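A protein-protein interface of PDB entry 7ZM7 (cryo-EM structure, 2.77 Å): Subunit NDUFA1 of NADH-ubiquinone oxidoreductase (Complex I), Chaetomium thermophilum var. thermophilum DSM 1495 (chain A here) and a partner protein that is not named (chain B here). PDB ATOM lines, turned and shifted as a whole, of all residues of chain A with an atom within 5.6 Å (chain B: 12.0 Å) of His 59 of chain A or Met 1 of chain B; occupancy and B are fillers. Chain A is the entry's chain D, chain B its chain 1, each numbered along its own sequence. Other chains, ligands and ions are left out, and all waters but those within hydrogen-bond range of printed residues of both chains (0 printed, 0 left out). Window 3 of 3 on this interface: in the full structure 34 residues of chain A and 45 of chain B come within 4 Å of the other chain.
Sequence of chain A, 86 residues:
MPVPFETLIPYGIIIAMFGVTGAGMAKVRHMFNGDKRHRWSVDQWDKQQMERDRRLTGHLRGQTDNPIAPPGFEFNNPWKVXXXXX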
ATOM      1  N   PHE A  32      -0.663  28.998 -11.068  1.00  0.00           N
ATOM      2  CA  PHE A  32       0.786  28.668 -10.980  1.00  0.00           C
ATOM      3  C   PHE A  32       1.598  29.944 -11.098  1.00  0.00           C
ATOM      4  O   PHE A  32       2.651  30.043 -10.461  1.00  0.00           O
ATOM      5  CB  PHE A  32       1.198  27.699 -12.088  1.00  0.00           C
ATOM      6  CG  PHE A  32       2.547  27.053 -11.917  1.00  0.00           C
ATOM      7  CD1 PHE A  32       2.865  26.377 -10.753  1.00  0.00           C
ATOM      8  CD2 PHE A  32       3.492  27.105 -12.927  1.00  0.00           C
ATOM      9  CE1 PHE A  32       4.101  25.771 -10.602  1.00  0.00           C
ATOM     10  CE2 PHE A  32       4.727  26.498 -12.774  1.00  0.00           C
ATOM     11  CZ  PHE A  32       5.028  25.831 -11.611  1.00  0.00           C
ATOM     12  N   ASN A  33       1.109  30.886 -11.904  1.00  0.00           N
ATOM     13  CA  ASN A  33       1.858  32.140 -12.171  1.00  0.00           C
ATOM     14  C   ASN A  33       1.448  33.247 -11.195  1.00  0.00           C
ATOM     15  O   ASN A  33       1.774  34.401 -11.471  1.00  0.00           O
ATOM     16  CB  ASN A  33       1.777  32.509 -13.651  1.00  0.00           C
ATOM     17  CG  ASN A  33       2.633  31.611 -14.515  1.00  0.00           C
ATOM     18  OD1 ASN A  33       3.842  31.796 -14.595  1.00  0.00           O
ATOM     19  ND2 ASN A  33       2.020  30.630 -15.152  1.00  0.00           N
ATOM     20  N   GLY A  34       0.766  32.914 -10.101  1.00  0.00           N
ATOM     21  CA  GLY A  34       0.476  33.918  -9.063  1.00  0.00           C
ATOM     22  C   GLY A  34      -0.805  34.640  -9.360  1.00  0.00           C
ATOM     23  O   GLY A  34      -0.874  35.853  -9.090  1.00  0.00           O
ATOM     24  N   LYS A  36      -1.919  35.507 -12.119  1.00  0.00           N
ATOM     25  CA  LYS A  36      -1.725  36.502 -13.197  1.00  0.00           C
ATOM     26  C   LYS A  36      -1.527  35.685 -14.467  1.00  0.00           C
ATOM     27  O   LYS A  36      -1.215  34.496 -14.340  1.00  0.00           O
ATOM     28  CB  LYS A  36      -0.582  37.467 -12.872  1.00  0.00           C
ATOM     29  CG  LYS A  36       0.829  36.964 -13.112  1.00  0.00           C
ATOM     30  CD  LYS A  36       1.837  37.862 -12.452  1.00  0.00           C
ATOM     31  CE  LYS A  36       1.522  38.101 -10.991  1.00  0.00           C
ATOM     32  NZ  LYS A  36       2.388  39.149 -10.404  1.00  0.00           N
ATOM     33  N   MET A  50      12.656  37.847 -15.297  1.00  0.00           N
ATOM     34  CA  MET A  50      11.896  37.125 -14.246  1.00  0.00           C
ATOM     35  C   MET A  50      12.815  36.724 -13.086  1.00  0.00           C
ATOM     36  O   MET A  50      12.343  36.733 -11.950  1.00  0.00           O
ATOM     37  CB  MET A  50      11.203  35.897 -14.821  1.00  0.00           C
ATOM     38  CG  MET A  50       9.910  36.230 -15.530  1.00  0.00           C
ATOM     39  SD  MET A  50       9.016  34.763 -16.078  1.00  0.00           S
ATOM     40  CE  MET A  50      10.027  34.267 -17.469  1.00  0.00           C
ATOM     41  N   ASP A  53      13.135  39.595 -11.040  1.00  0.00           N
ATOM     42  CA  ASP A  53      11.892  39.755 -10.296  1.00  0.00           C
ATOM     43  C   ASP A  53      11.901  38.906  -9.044  1.00  0.00           C
ATOM     44  O   ASP A  53      11.403  39.328  -7.998  1.00  0.00           O
ATOM     45  CB  ASP A  53      10.702  39.360 -11.162  1.00  0.00           C
ATOM     46  CG  ASP A  53      10.520  40.256 -12.342  1.00  0.00           C
ATOM     47  OD1 ASP A  53      11.307  41.207 -12.495  1.00  0.00           O
ATOM     48  OD2 ASP A  53       9.574  40.012 -13.118  1.00  0.00           O
ATOM     49  N   ARG A  54      12.433  37.687  -9.144  1.00  0.00           N
ATOM     50  CA  ARG A  54      12.581  36.838  -7.973  1.00  0.00           C
ATOM     51  C   ARG A  54      13.523  37.460  -6.968  1.00  0.00           C
ATOM     52  O   ARG A  54      13.299  37.355  -5.763  1.00  0.00           O
ATOM     53  CB  ARG A  54      13.079  35.458  -8.375  1.00  0.00           C
ATOM     54  CG  ARG A  54      13.220  34.510  -7.204  1.00  0.00           C
ATOM     55  CD  ARG A  54      12.972  33.099  -7.616  1.00  0.00           C
ATOM     56  NE  ARG A  54      13.980  32.657  -8.556  1.00  0.00           N
ATOM     57  CZ  ARG A  54      13.999  31.458  -9.108  1.00  0.00           C
ATOM     58  NH1 ARG A  54      14.952  31.135  -9.957  1.00  0.00           N
ATOM     59  NH2 ARG A  54      13.061  30.585  -8.803  1.00  0.00           N
ATOM     60  N   THR A  57      11.423  40.311  -5.214  1.00  0.00           N
ATOM     61  CA  THR A  57      10.221  39.898  -4.506  1.00  0.00           C
ATOM     62  C   THR A  57      10.260  38.484  -3.953  1.00  0.00           C
ATOM     63  O   THR A  57       9.563  38.206  -2.983  1.00  0.00           O
ATOM     64  CB  THR A  57       8.993  40.008  -5.415  1.00  0.00           C
ATOM     65  OG1 THR A  57       8.978  38.902  -6.317  1.00  0.00           O
ATOM     66  CG2 THR A  57       9.009  41.313  -6.192  1.00  0.00           C
ATOM     67  N   GLY A  58      10.971  37.565  -4.603  1.00  0.00           N
ATOM     68  CA  GLY A  58      10.948  36.144  -4.199  1.00  0.00           C
ATOM     69  C   GLY A  58      10.113  35.322  -5.163  1.00  0.00           C
ATOM     70  O   GLY A  58      10.302  34.107  -5.204  1.00  0.00           O
ATOM     71  N   HIS A  59       9.261  35.978  -5.951  1.00  0.00           N
ATOM     72  CA  HIS A  59       8.409  35.290  -6.956  1.00  0.00           C
ATOM     73  C   HIS A  59       8.903  35.662  -8.355  1.00  0.00           C
ATOM     74  O   HIS A  59       9.161  36.844  -8.584  1.00  0.00           O
ATOM     75  CB  HIS A  59       6.941  35.646  -6.701  1.00  0.00           C
ATOM     76  CG  HIS A  59       5.934  34.921  -7.531  1.00  0.00           C
ATOM     77  ND1 HIS A  59       6.257  33.868  -8.362  1.00  0.00           N
ATOM     78  CD2 HIS A  59       4.600  35.089  -7.646  1.00  0.00           C
ATOM     79  CE1 HIS A  59       5.169  33.429  -8.959  1.00  0.00           C
ATOM     80  NE2 HIS A  59       4.140  34.156  -8.534  1.00  0.00           N
ATOM     81  N   LEU A  60       9.018  34.683  -9.249  1.00  0.00           N
ATOM     82  CA  LEU A  60       9.471  34.921 -10.643  1.00  0.00           C
ATOM     83  C   LEU A  60       8.496  35.865 -11.349  1.00  0.00           C
ATOM     84  O   LEU A  60       8.953  36.606 -12.230  1.00  0.00           O
ATOM     85  CB  LEU A  60       9.574  33.575 -11.365  1.00  0.00           C
ATOM     86  CG  LEU A  60      10.778  32.712 -11.000  1.00  0.00           C
ATOM     87  CD1 LEU A  60      10.518  31.257 -11.347  1.00  0.00           C
ATOM     88  CD2 LEU A  60      12.030  33.212 -11.700  1.00  0.00           C
ATOM     89  N   ARG A  61       7.207  35.822 -10.997  1.00  0.00           N
ATOM     90  CA  ARG A  61       6.211  36.758 -11.581  1.00  0.00           C
ATOM     91  C   ARG A  61       5.984  38.008 -10.717  1.00  0.00           C
ATOM     92  O   ARG A  61       5.133  38.818 -11.113  1.00  0.00           O
ATOM     93  CB  ARG A  61       4.891  36.041 -11.852  1.00  0.00           C
ATOM     94  CG  ARG A  61       5.011  34.851 -12.791  1.00  0.00           C
ATOM     95  CD  ARG A  61       5.557  35.258 -14.144  1.00  0.00           C
ATOM     96  NE  ARG A  61       4.837  36.391 -14.704  1.00  0.00           N
ATOM     97  CZ  ARG A  61       3.754  36.296 -15.461  1.00  0.00           C
ATOM     98  NH1 ARG A  61       3.171  37.386 -15.924  1.00  0.00           N
ATOM     99  NH2 ARG A  61       3.255  35.110 -15.752  1.00  0.00           N
ATOM    100  N   GLY A  62       6.699  38.181  -9.604  1.00  0.00           N
ATOM    101  CA  GLY A  62       6.444  39.328  -8.706  1.00  0.00           C
ATOM    102  C   GLY A  62       6.811  40.679  -9.303  1.00  0.00           C
ATOM    103  O   GLY A  62       7.838  40.739  -9.992  1.00  0.00           O
ATOM    104  N   MET B   1       7.101  30.658  -8.223  1.00  0.00           N
ATOM    105  CA  MET B   1       5.871  29.963  -8.683  1.00  0.00           C
ATOM    106  C   MET B   1       5.003  29.582  -7.481  1.00  0.00           C
ATOM    107  O   MET B   1       5.576  29.269  -6.426  1.00  0.00           O
ATOM    108  CB  MET B   1       6.205  28.757  -9.555  1.00  0.00           C
ATOM    109  CG  MET B   1       6.807  29.155 -10.890  1.00  0.00           C
ATOM    110  SD  MET B   1       5.685  30.177 -11.883  1.00  0.00           S
ATOM    111  CE  MET B   1       6.850  31.110 -12.872  1.00  0.00           C
ATOM    112  N   SER B   2       3.680  29.640  -7.623  1.00  0.00           N
ATOM    113  CA  SER B   2       2.756  29.434  -6.481  1.00  0.00           C
ATOM    114  C   SER B   2       2.752  28.016  -5.900  1.00  0.00           C
ATOM    115  O   SER B   2       2.766  27.897  -4.663  1.00  0.00           O
ATOM    116  CB  SER B   2       1.388  29.892  -6.860  1.00  0.00           C
ATOM    117  OG  SER B   2       1.455  31.174  -7.465  1.00  0.00           O
ATOM    118  N   TYR B   3       2.728  26.982  -6.739  1.00  0.00           N
ATOM    119  CA  TYR B   3       2.806  25.604  -6.202  1.00  0.00           C
ATOM    120  C   TYR B   3       3.987  24.861  -6.823  1.00  0.00           C
ATOM    121  O   TYR B   3       4.731  25.476  -7.588  1.00  0.00           O
ATOM    122  CB  TYR B   3       1.466  24.878  -6.327  1.00  0.00           C
ATOM    123  CG  TYR B   3       0.823  24.870  -7.690  1.00  0.00           C
ATOM    124  CD1 TYR B   3      -0.051  25.871  -8.074  1.00  0.00           C
ATOM    125  CD2 TYR B   3       1.053  23.835  -8.580  1.00  0.00           C
ATOM    126  CE1 TYR B   3      -0.661  25.861  -9.316  1.00  0.00           C
ATOM    127  CE2 TYR B   3       0.452  23.811  -9.828  1.00  0.00           C
ATOM    128  CZ  TYR B   3      -0.406  24.829 -10.198  1.00  0.00           C
ATOM    129  OH  TYR B   3      -1.001  24.813 -11.424  1.00  0.00           O
ATOM    130  N   SER B   4       4.145  23.572  -6.538  1.00  0.00           N
ATOM    131  CA  SER B   4       5.281  22.769  -7.053  1.00  0.00           C
ATOM    132  C   SER B   4       5.172  22.495  -8.553  1.00  0.00           C
ATOM    133  O   SER B   4       4.047  22.311  -9.035  1.00  0.00           O
ATOM    134  CB  SER B   4       5.356  21.505  -6.292  1.00  0.00           C
ATOM    135  OG  SER B   4       4.068  20.924  -6.170  1.00  0.00           O
ATOM    136  N   GLN B   5       6.309  22.434  -9.250  1.00  0.00           N
ATOM    137  CA  GLN B   5       6.353  22.202 -10.717  1.00  0.00           C
ATOM    138  C   GLN B   5       5.800  20.826 -11.078  1.00  0.00           C
ATOM    139  O   GLN B   5       5.073  20.751 -12.050  1.00  0.00           O
ATOM    140  CB  GLN B   5       7.792  22.315 -11.217  1.00  0.00           C
ATOM    141  CG  GLN B   5       8.103  23.665 -11.840  1.00  0.00           C
ATOM    142  CD  GLN B   5       9.462  23.683 -12.489  1.00  0.00           C
ATOM    143  OE1 GLN B   5      10.326  22.861 -12.189  1.00  0.00           O
ATOM    144  NE2 GLN B   5       9.658  24.629 -13.392  1.00  0.00           N
ATOM    145  N   THR B   6       6.115  19.793 -10.312  1.00  0.00           N
ATOM    146  CA  THR B   6       5.685  18.413 -10.629  1.00  0.00           C
ATOM    147  C   THR B   6       4.168  18.353 -10.620  1.00  0.00           C
ATOM    148  O   THR B   6       3.624  17.720 -11.535  1.00  0.00           O
ATOM    149  CB  THR B   6       6.327  17.391  -9.683  1.00  0.00           C
ATOM    150  OG1 THR B   6       7.731  17.376  -9.941  1.00  0.00           O
ATOM    151  CG2 THR B   6       5.773  15.992  -9.835  1.00  0.00           C
ATOM    152  N   ILE B   7       3.504  18.979  -9.647  1.00  0.00           N
ATOM    153  CA  ILE B   7       2.048  19.043  -9.702  1.00  0.00           C
ATOM    154  C   ILE B   7       1.588  19.753 -10.968  1.00  0.00           C
ATOM    155  O   ILE B   7       0.724  19.255 -11.695  1.00  0.00           O
ATOM    156  CB  ILE B   7       1.490  19.721  -8.442  1.00  0.00           C
ATOM    157  CG1 ILE B   7       1.819  18.896  -7.203  1.00  0.00           C
ATOM    158  CG2 ILE B   7       0.008  19.935  -8.570  1.00  0.00           C
ATOM    159  CD1 ILE B   7       1.100  17.572  -7.151  1.00  0.00           C
ATOM    160  N   ASN B   8       2.158  20.925 -11.251  1.00  0.00           N
ATOM    161  CA  ASN B   8       1.789  21.643 -12.466  1.00  0.00           C
ATOM    162  C   ASN B   8       2.078  20.802 -13.698  1.00  0.00           C
ATOM    163  O   ASN B   8       1.247  20.706 -14.605  1.00  0.00           O
ATOM    164  CB  ASN B   8       2.539  22.973 -12.537  1.00  0.00           C
ATOM    165  CG  ASN B   8       1.969  23.920 -13.577  1.00  0.00           C
ATOM    166  OD1 ASN B   8       0.904  24.478 -13.394  1.00  0.00           O
ATOM    167  ND2 ASN B   8       2.678  24.099 -14.665  1.00  0.00           N
ATOM    168  N   SER B   9       3.236  20.160 -13.737  1.00  0.00           N
ATOM    169  CA  SER B   9       3.547  19.254 -14.868  1.00  0.00           C
ATOM    170  C   SER B   9       2.434  18.210 -14.993  1.00  0.00           C
ATOM    171  O   SER B   9       1.892  18.075 -16.097  1.00  0.00           O
ATOM    172  CB  SER B   9       4.893  18.622 -14.676  1.00  0.00           C
ATOM    173  OG  SER B   9       5.900  19.609 -14.531  1.00  0.00           O
ATOM    174  N   GLU B  12      -1.257  19.543 -16.306  1.00  0.00           N
ATOM    175  CA  GLU B  12      -1.333  19.914 -17.739  1.00  0.00           C
ATOM    176  C   GLU B  12      -1.269  18.662 -18.620  1.00  0.00           C
ATOM    177  O   GLU B  12      -2.026  18.579 -19.593  1.00  0.00           O
ATOM    178  CB  GLU B  12      -0.311  20.990 -18.092  1.00  0.00           C
ATOM    179  CG  GLU B  12      -0.537  22.275 -17.328  1.00  0.00           C
ATOM    180  CD  GLU B  12       0.662  23.196 -17.253  1.00  0.00           C
ATOM    181  OE1 GLU B  12       1.636  22.966 -17.986  1.00  0.00           O
ATOM    182  OE2 GLU B  12       0.614  24.138 -16.452  1.00  0.00           O
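N of Ser 2 of chain B sits at hydrogen-bond distance from O of Phe 32 of chain A, at 3.0 Å.
ND1 of His 59 of chain A lies within hydrogen-bond range of N of Met 1 of chain B, 3.3 Å away.
The side-chain sulfur of Met 1 of chain B sits close to the side-chain amide oxygen of Asn 33 of chain A (3.7 Å).
The side-chain sulfur of Met 1 of chain B lies close to the backbone carbonyl oxygen of Phe 32 of chain A, at 3.4 Å.
OG of Ser 2 of chain B is in hydrogen-bond range of N of Gly 34 of chain A, at 3.2 Å.
O of His 59 of chain A is in hydrogen-bond range of N of Arg 54 of chain A (3.4 Å).
OH of Tyr 3 of chain B is in hydrogen-bond range of OD1 of Asn 8 of chain B (2.8 Å).
The side-chain amide nitrogen of Asn 8 of chain B is in hydrogen-bond range of the side-chain carboxylate of Glu 12 of chain B (2.7 Å).
The backbone carbonyl oxygen (O) of Gln 5 of chain B is in hydrogen-bond range of the side-chain hydroxyl (OG) of Ser 9 of chain B, 2.9 Å away.
N of His 59 of chain A is in hydrogen-bond range of OG1 of Thr 57 of chain A (3.0 Å).
A ring nitrogen (ND1) of His 59 of chain A sits close to the backbone NH of Arg 61 of chain A (3.4 Å).
Among the printed residues, pairs that only touch across the chains: Phe 32 of chain A with Tyr 3 of chain B (3.1 Å), Phe 32 of chain A with Asn 8 of chain B (3.4 Å), Phe 32 of chain A with Gln 5 of chain B (3.8 Å), Phe 32 of chain A with Ser 4 of chain B (3.8 Å) and Leu 60 of chain A with Met 1 of chain B (3.97 Å).
Phe 32 of chain A touches just these residues of chain B: Met 1 (3.4 Å), Ser 2 (3.0 Å), Tyr 3 (3.1 Å), Ser 4 (3.8 Å), Gln 5 (3.8 Å) and Asn 8 (3.4 Å).
Of chain B, only Met 1 comes within 4 Å of Asn 33 of chain A.
Of chain B, only Ser 2 comes within 4 Å of Gly 34 of chain A.
No residue of chain B comes within 4 Å of Met 50 of chain A.
No residue of chain B comes within 4 Å of Gly 58 of chain A.
Printed residues of chain B within 4 Å of His 59 of chain A: Met 1 (3.3 Å).
Leu 60 of chain A touches one residue of chain B.
Arg 61 of chain A touches none of the printed residues of chain B.
Gly 62 of chain A touches none of the printed residues of chain B.
Of chain A, only Phe 32, Asn 33, His 59 and Leu 60 come within 4 Å of Met 1 of chain B.
Printed residues of chain A within 4 Å of Ser 2 of chain B: Phe 32 and Gly 34.
Of the printed residues of chain A, Ser 4 of chain B touches Phe 32 (3.8 Å).
Of the printed residues of chain A, Gln 5 of chain B touches Phe 32 (3.8 Å).
Ile 7 of chain B touches none of the printed residues of chain A.
The nearest residue of chain B that does not touch His 59 of chain A is Ser 2 of chain B (4.2 Å).
Hydrophobic or aromatic side chains of chain B that line the printed part of chain A: Met 1 and Tyr 3.
Of the 13 printed residues of chain A, 5 touch a printed residue of chain B.
Among the printed residues, 10 pairs touch across the chains.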
